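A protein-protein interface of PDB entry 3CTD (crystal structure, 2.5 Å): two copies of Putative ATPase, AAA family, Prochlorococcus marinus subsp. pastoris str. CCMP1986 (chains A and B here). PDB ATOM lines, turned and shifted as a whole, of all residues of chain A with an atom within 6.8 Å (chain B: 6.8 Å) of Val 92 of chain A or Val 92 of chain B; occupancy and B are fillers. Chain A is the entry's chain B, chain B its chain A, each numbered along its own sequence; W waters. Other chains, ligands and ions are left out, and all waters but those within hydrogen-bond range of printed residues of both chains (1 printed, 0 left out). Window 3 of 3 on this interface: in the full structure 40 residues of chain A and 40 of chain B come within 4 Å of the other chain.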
ATOM      1  N   LEU A  76      12.915  38.903 -23.355  1.00  0.00           N
ATOM      2  CA  LEU A  76      13.626  37.629 -23.305  1.00  0.00           C
ATOM      3  C   LEU A  76      13.165  36.878 -22.059  1.00  0.00           C
ATOM      4  O   LEU A  76      12.747  35.716 -22.144  1.00  0.00           O
ATOM      5  CB  LEU A  76      15.144  37.790 -23.309  1.00  0.00           C
ATOM      6  CG  LEU A  76      15.827  38.195 -24.635  1.00  0.00           C
ATOM      7  CD1 LEU A  76      17.252  38.748 -24.353  1.00  0.00           C
ATOM      8  CD2 LEU A  76      15.869  37.083 -25.694  1.00  0.00           C
ATOM      9  N   ALA A  79       9.641  35.577 -22.387  1.00  0.00           N
ATOM     10  CA  ALA A  79       9.634  34.384 -23.231  1.00  0.00           C
ATOM     11  C   ALA A  79       9.903  33.056 -22.487  1.00  0.00           C
ATOM     12  O   ALA A  79       9.522  31.975 -22.947  1.00  0.00           O
ATOM     13  CB  ALA A  79      10.621  34.575 -24.406  1.00  0.00           C
ATOM     14  N   ASP A  87       5.829  27.128 -25.668  1.00  0.00           N
ATOM     15  CA  ASP A  87       6.478  27.228 -26.977  1.00  0.00           C
ATOM     16  C   ASP A  87       7.958  27.598 -26.772  1.00  0.00           C
ATOM     17  O   ASP A  87       8.328  28.775 -26.746  1.00  0.00           O
ATOM     18  CB  ASP A  87       5.754  28.253 -27.869  1.00  0.00           C
ATOM     19  CG  ASP A  87       6.463  28.491 -29.225  1.00  0.00           C
ATOM     20  OD1 ASP A  87       7.346  27.706 -29.623  1.00  0.00           O
ATOM     21  OD2 ASP A  87       6.156  29.501 -29.896  1.00  0.00           O
ATOM     22  N   PRO A  88       8.818  26.584 -26.641  1.00  0.00           N
ATOM     23  CA  PRO A  88      10.196  26.914 -26.319  1.00  0.00           C
ATOM     24  C   PRO A  88      10.922  27.584 -27.496  1.00  0.00           C
ATOM     25  O   PRO A  88      12.050  27.991 -27.351  1.00  0.00           O
ATOM     26  CB  PRO A  88      10.811  25.561 -25.978  1.00  0.00           C
ATOM     27  CG  PRO A  88       9.952  24.548 -26.680  1.00  0.00           C
ATOM     28  CD  PRO A  88       8.609  25.138 -26.905  1.00  0.00           C
ATOM     29  N   ASN A  89      10.277  27.718 -28.645  1.00  0.00           N
ATOM     30  CA  ASN A  89      10.870  28.464 -29.753  1.00  0.00           C
ATOM     31  C   ASN A  89      10.778  29.993 -29.528  1.00  0.00           C
ATOM     32  O   ASN A  89      11.533  30.799 -30.110  1.00  0.00           O
ATOM     33  CB  ASN A  89      10.198  28.032 -31.076  1.00  0.00           C
ATOM     34  CG  ASN A  89      10.920  28.576 -32.312  1.00  0.00           C
ATOM     35  OD1 ASN A  89      12.093  28.283 -32.546  1.00  0.00           O
ATOM     36  ND2 ASN A  89      10.206  29.366 -33.115  1.00  0.00           N
ATOM     37  N   ALA A  90       9.856  30.402 -28.657  1.00  0.00           N
ATOM     38  CA  ALA A  90       9.639  31.817 -28.386  1.00  0.00           C
ATOM     39  C   ALA A  90      10.943  32.511 -28.020  1.00  0.00           C
ATOM     40  O   ALA A  90      11.178  33.636 -28.465  1.00  0.00           O
ATOM     41  CB  ALA A  90       8.558  32.016 -27.258  1.00  0.00           C
ATOM     42  N   ILE A  91      11.773  31.864 -27.192  1.00  0.00           N
ATOM     43  CA  ILE A  91      13.043  32.481 -26.812  1.00  0.00           C
ATOM     44  C   ILE A  91      13.953  32.608 -28.033  1.00  0.00           C
ATOM     45  O   ILE A  91      14.671  33.570 -28.135  1.00  0.00           O
ATOM     46  CB  ILE A  91      13.761  31.791 -25.598  1.00  0.00           C
ATOM     47  CG1 ILE A  91      14.954  32.601 -25.125  1.00  0.00           C
ATOM     48  CG2 ILE A  91      14.252  30.395 -25.934  1.00  0.00           C
ATOM     49  CD1 ILE A  91      14.561  33.712 -24.229  1.00  0.00           C
ATOM     50  N   VAL A  92      13.888  31.665 -28.972  1.00  0.00           N
ATOM     51  CA  VAL A  92      14.710  31.772 -30.171  1.00  0.00           C
ATOM     52  C   VAL A  92      14.251  32.949 -31.025  1.00  0.00           C
ATOM     53  O   VAL A  92      15.067  33.682 -31.537  1.00  0.00           O
ATOM     54  CB  VAL A  92      14.651  30.470 -31.021  1.00  0.00           C
ATOM     55  CG1 VAL A  92      15.471  30.618 -32.343  1.00  0.00           C
ATOM     56  CG2 VAL A  92      15.071  29.222 -30.187  1.00  0.00           C
ATOM     57  N   VAL A  93      12.940  33.138 -31.174  1.00  0.00           N
ATOM     58  CA  VAL A  93      12.424  34.181 -32.054  1.00  0.00           C
ATOM     59  C   VAL A  93      12.764  35.567 -31.475  1.00  0.00           C
ATOM     60  O   VAL A  93      13.238  36.467 -32.187  1.00  0.00           O
ATOM     61  CB  VAL A  93      10.873  34.029 -32.267  1.00  0.00           C
ATOM     62  CG1 VAL A  93      10.233  35.299 -32.909  1.00  0.00           C
ATOM     63  CG2 VAL A  93      10.543  32.758 -33.078  1.00  0.00           C
ATOM     64  N   VAL A  94      12.487  35.753 -30.197  1.00  0.00           N
ATOM     65  CA  VAL A  94      12.741  37.026 -29.551  1.00  0.00           C
ATOM     66  C   VAL A  94      14.231  37.356 -29.544  1.00  0.00           C
ATOM     67  O   VAL A  94      14.597  38.502 -29.718  1.00  0.00           O
ATOM     68  CB  VAL A  94      12.288  37.004 -28.084  1.00  0.00           C
ATOM     69  CG1 VAL A  94      12.809  38.219 -27.402  1.00  0.00           C
ATOM     70  CG2 VAL A  94      10.776  36.911 -28.005  1.00  0.00           C
ATOM     71  N   GLN A  95      15.085  36.346 -29.335  1.00  0.00           N
ATOM     72  CA  GLN A  95      16.519  36.567 -29.320  1.00  0.00           C
ATOM     73  C   GLN A  95      16.970  37.031 -30.689  1.00  0.00           C
ATOM     74  O   GLN A  95      17.799  37.914 -30.843  1.00  0.00           O
ATOM     75  CB  GLN A  95      17.288  35.315 -28.880  1.00  0.00           C
ATOM     76  CG  GLN A  95      18.790  35.440 -29.062  1.00  0.00           C
ATOM     77  CD  GLN A  95      19.357  36.547 -28.213  1.00  0.00           C
ATOM     78  OE1 GLN A  95      19.024  36.675 -27.009  1.00  0.00           O
ATOM     79  NE2 GLN A  95      20.225  37.371 -28.814  1.00  0.00           N
ATOM     80  N   SER A  96      16.366  36.448 -31.689  1.00  0.00           N
ATOM     81  CA  SER A  96      16.649  36.809 -33.047  1.00  0.00           C
ATOM     82  C   SER A  96      16.117  38.214 -33.454  1.00  0.00           C
ATOM     83  O   SER A  96      16.746  38.903 -34.239  1.00  0.00           O
ATOM     84  CB  SER A  96      16.038  35.705 -33.915  1.00  0.00           C
ATOM     85  OG  SER A  96      16.136  36.002 -35.273  1.00  0.00           O
ATOM     86  N   CYS A  97      14.956  38.624 -32.927  1.00  0.00           N
ATOM     87  CA  CYS A  97      14.498  40.006 -32.975  1.00  0.00           C
ATOM     88  C   CYS A  97      15.522  40.956 -32.341  1.00  0.00           C
ATOM     89  O   CYS A  97      15.900  41.960 -32.963  1.00  0.00           O
ATOM     90  CB  CYS A  97      13.143  40.125 -32.280  1.00  0.00           C
ATOM     91  SG  CYS A  97      11.815  39.344 -33.249  1.00  0.00           S
ATOM     92  N   LEU B  76      24.792  22.616 -23.349  1.00  0.00           N
ATOM     93  CA  LEU B  76      25.078  22.608 -24.802  1.00  0.00           C
ATOM     94  C   LEU B  76      25.539  21.285 -25.259  1.00  0.00           C
ATOM     95  O   LEU B  76      25.054  20.769 -26.255  1.00  0.00           O
ATOM     96  CB  LEU B  76      26.238  23.482 -25.135  1.00  0.00           C
ATOM     97  CG  LEU B  76      25.880  24.858 -25.512  1.00  0.00           C
ATOM     98  CD1 LEU B  76      27.189  25.383 -26.049  1.00  0.00           C
ATOM     99  CD2 LEU B  76      24.759  24.780 -26.554  1.00  0.00           C
ATOM    100  N   ALA B  79      22.796  18.884 -25.159  1.00  0.00           N
ATOM    101  CA  ALA B  79      21.846  19.093 -26.226  1.00  0.00           C
ATOM    102  C   ALA B  79      22.297  18.387 -27.488  1.00  0.00           C
ATOM    103  O   ALA B  79      21.508  18.034 -28.377  1.00  0.00           O
ATOM    104  CB  ALA B  79      21.643  20.552 -26.488  1.00  0.00           C
ATOM    105  N   PRO B  88      16.766  18.105 -33.365  1.00  0.00           N
ATOM    106  CA  PRO B  88      17.956  18.814 -33.782  1.00  0.00           C
ATOM    107  C   PRO B  88      17.873  20.317 -33.464  1.00  0.00           C
ATOM    108  O   PRO B  88      18.874  21.007 -33.578  1.00  0.00           O
ATOM    109  CB  PRO B  88      17.997  18.566 -35.272  1.00  0.00           C
ATOM    110  CG  PRO B  88      17.006  17.531 -35.562  1.00  0.00           C
ATOM    111  CD  PRO B  88      16.045  17.454 -34.464  1.00  0.00           C
ATOM    112  N   ASN B  89      16.709  20.815 -33.035  1.00  0.00           N
ATOM    113  CA  ASN B  89      16.644  22.205 -32.583  1.00  0.00           C
ATOM    114  C   ASN B  89      17.009  22.409 -31.090  1.00  0.00           C
ATOM    115  O   ASN B  89      17.149  23.563 -30.625  1.00  0.00           O
ATOM    116  CB  ASN B  89      15.306  22.865 -32.971  1.00  0.00           C
ATOM    117  CG  ASN B  89      15.119  22.919 -34.488  1.00  0.00           C
ATOM    118  OD1 ASN B  89      14.569  21.981 -35.098  1.00  0.00           O
ATOM    119  ND2 ASN B  89      15.637  23.970 -35.110  1.00  0.00           N
ATOM    120  N   ALA B  90      17.264  21.305 -30.379  1.00  0.00           N
ATOM    121  CA  ALA B  90      17.717  21.404 -28.986  1.00  0.00           C
ATOM    122  C   ALA B  90      18.925  22.316 -28.789  1.00  0.00           C
ATOM    123  O   ALA B  90      18.919  23.166 -27.875  1.00  0.00           O
ATOM    124  CB  ALA B  90      17.922  20.000 -28.354  1.00  0.00           C
ATOM    125  N   ILE B  91      19.937  22.225 -29.661  1.00  0.00           N
ATOM    126  CA  ILE B  91      21.087  23.157 -29.534  1.00  0.00           C
ATOM    127  C   ILE B  91      20.740  24.602 -29.852  1.00  0.00           C
ATOM    128  O   ILE B  91      21.472  25.568 -29.426  1.00  0.00           O
ATOM    129  CB  ILE B  91      22.292  22.804 -30.427  1.00  0.00           C
ATOM    130  CG1 ILE B  91      21.807  22.251 -31.773  1.00  0.00           C
ATOM    131  CG2 ILE B  91      23.265  21.875 -29.692  1.00  0.00           C
ATOM    132  CD1 ILE B  91      22.681  22.657 -32.908  1.00  0.00           C
ATOM    133  N   VAL B  92      19.668  24.783 -30.634  1.00  0.00           N
ATOM    134  CA  VAL B  92      19.266  26.134 -30.966  1.00  0.00           C
ATOM    135  C   VAL B  92      18.643  26.777 -29.706  1.00  0.00           C
ATOM    136  O   VAL B  92      19.057  27.843 -29.264  1.00  0.00           O
ATOM    137  CB  VAL B  92      18.247  26.183 -32.177  1.00  0.00           C
ATOM    138  CG1 VAL B  92      17.948  27.648 -32.533  1.00  0.00           C
ATOM    139  CG2 VAL B  92      18.746  25.373 -33.407  1.00  0.00           C
ATOM    140  N   VAL B  93      17.660  26.105 -29.118  1.00  0.00           N
ATOM    141  CA  VAL B  93      16.990  26.603 -27.928  1.00  0.00           C
ATOM    142  C   VAL B  93      17.985  26.888 -26.819  1.00  0.00           C
ATOM    143  O   VAL B  93      17.956  27.983 -26.217  1.00  0.00           O
ATOM    144  CB  VAL B  93      15.888  25.611 -27.489  1.00  0.00           C
ATOM    145  CG1 VAL B  93      15.210  26.002 -26.119  1.00  0.00           C
ATOM    146  CG2 VAL B  93      14.888  25.467 -28.647  1.00  0.00           C
ATOM    147  N   VAL B  94      18.865  25.919 -26.523  1.00  0.00           N
ATOM    148  CA  VAL B  94      19.885  26.066 -25.452  1.00  0.00           C
ATOM    149  C   VAL B  94      20.854  27.238 -25.714  1.00  0.00           C
ATOM    150  O   VAL B  94      21.143  28.054 -24.793  1.00  0.00           O
ATOM    151  CB  VAL B  94      20.690  24.734 -25.250  1.00  0.00           C
ATOM    152  CG1 VAL B  94      21.831  24.938 -24.328  1.00  0.00           C
ATOM    153  CG2 VAL B  94      19.759  23.569 -24.806  1.00  0.00           C
ATOM    154  N   GLN B  95      21.355  27.374 -26.946  1.00  0.00           N
ATOM    155  CA  GLN B  95      22.109  28.612 -27.245  1.00  0.00           C
ATOM    156  C   GLN B  95      21.356  29.933 -27.063  1.00  0.00           C
ATOM    157  O   GLN B  95      21.922  30.938 -26.560  1.00  0.00           O
ATOM    158  CB  GLN B  95      22.818  28.558 -28.606  1.00  0.00           C
ATOM    159  CG  GLN B  95      24.245  28.122 -28.371  1.00  0.00           C
ATOM    160  CD  GLN B  95      24.874  27.547 -29.565  1.00  0.00           C
ATOM    161  OE1 GLN B  95      24.322  26.671 -30.190  1.00  0.00           O
ATOM    162  NE2 GLN B  95      26.063  28.006 -29.885  1.00  0.00           N
ATOM    163  N   SER B  96      20.093  29.968 -27.469  1.00  0.00           N
ATOM    164  CA  SER B  96      19.319  31.174 -27.175  1.00  0.00           C
ATOM    165  C   SER B  96      19.219  31.365 -25.684  1.00  0.00           C
ATOM    166  O   SER B  96      19.367  32.472 -25.210  1.00  0.00           O
ATOM    167  CB  SER B  96      17.935  31.157 -27.813  1.00  0.00           C
ATOM    168  OG  SER B  96      17.967  30.851 -29.210  1.00  0.00           O
ATOM    169  N   CYS B  97      18.983  30.315 -24.911  1.00  0.00           N
ATOM    170  CA  CYS B  97      18.981  30.524 -23.463  1.00  0.00           C
ATOM    171  C   CYS B  97      20.307  31.044 -22.918  1.00  0.00           C
ATOM    172  O   CYS B  97      20.244  31.850 -21.997  1.00  0.00           O
ATOM    173  CB  CYS B  97      18.561  29.281 -22.664  1.00  0.00           C
ATOM    174  SG  CYS B  97      16.893  28.697 -22.967  1.00  0.00           S
ATOM    175  N   GLN B 115      14.491  26.914 -18.161  1.00  0.00           N
ATOM    176  CA  GLN B 115      13.882  26.453 -19.426  1.00  0.00           C
ATOM    177  C   GLN B 115      14.784  25.454 -20.203  1.00  0.00           C
ATOM    178  O   GLN B 115      14.338  24.470 -20.768  1.00  0.00           O
ATOM    179  CB  GLN B 115      13.400  27.616 -20.322  1.00  0.00           C
ATOM    180  CG  GLN B 115      13.323  27.231 -21.851  1.00  0.00           C
ATOM    181  CD  GLN B 115      12.309  28.065 -22.594  1.00  0.00           C
ATOM    182  OE1 GLN B 115      11.497  28.733 -21.969  1.00  0.00           O
ATOM    183  NE2 GLN B 115      12.346  28.038 -23.918  1.00  0.00           N
HETATM  184  O   HOH W   1      10.268  30.162 -25.053  1.00  0.00           O
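The side-chain amide nitrogen of Gln 115 of chain B sits close to the backbone carbonyl oxygen of Pro 88 of chain A (3.4 Å).
O of Val 93 of chain B lies within hydrogen-bond range of SG of Cys 97 of chain B, at 3.5 Å. O of Val 92 of chain B is in hydrogen-bond range of OG of Ser 96 of chain B.
Among the printed residues, merely in contact across the chains: Val 92 of chain A with Ser 96 of chain B, Ile 91 of chain A with Gln 115 of chain B, Val 92 of chain A with Val 92 of chain B, Ala 79 of chain A with Gln 115 of chain B, Pro 88 of chain A with Val 93 of chain B and Val 92 of chain A with Val 93 of chain B.
Val 92 of chain A touches just these residues of chain B: Val 92, Val 93 and Ser 96. Val 92 of chain B touches just one residue of chain A: Val 92. Printed residues of chain B within 4 Å of Ala 79 of chain A: Gln 115. Of the printed residues of chain A, Gln 115 of chain B touches Ala 79 (3.9 Å), Pro 88 (3.4 Å) and Ile 91 (3.6 Å). Of the printed residues of chain A, Val 93 of chain B touches Pro 88 and Val 92. Asp 87 of chain A touches none of the printed residues of chain B. The nearest residue of chain A that does not touch Val 92 of chain B is Asn 89 of chain A (5.9 Å).
Printed residues of chain A that touch a printed residue of chain B: Ala 79, Pro 88, Ile 91 and Val 92. Hydrophobic or aromatic side chains of chain A within 4 Å of the printed part of chain B: Pro 88, Ile 91 and Val 92.
Pro 88 of chain A touches Val 93 of chain B, but with the chains exchanged Val 93 of chain A does not touch Pro 88 of chain B (13.7 Å). Val 92 of chain A touches its own counterpart, Val 92 of chain B. Val 92 of chain A touches Val 93 of chain B, but with the chains exchanged Val 93 of chain A does not touch Val 92 of chain B (7.6 Å). Val 92 of chain A touches Ser 96 of chain B, but with the chains exchanged Ser 96 of chain A does not touch Val 92 of chain B (8.4 Å). Of the 7 pairs that touch across the chains among the printed residues, 1 has its exchanged pair printed and touching as well.
Water W1 lies within hydrogen-bond range of the backbone carbonyl oxygen (O) of Ala 79 of chain A, the backbone carbonyl oxygen (O) of Asp 87 of chain A, the backbone NH (N) of Ile 91 of chain A and the side-chain amide nitrogen (NE2) of Gln 115 of chain B.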
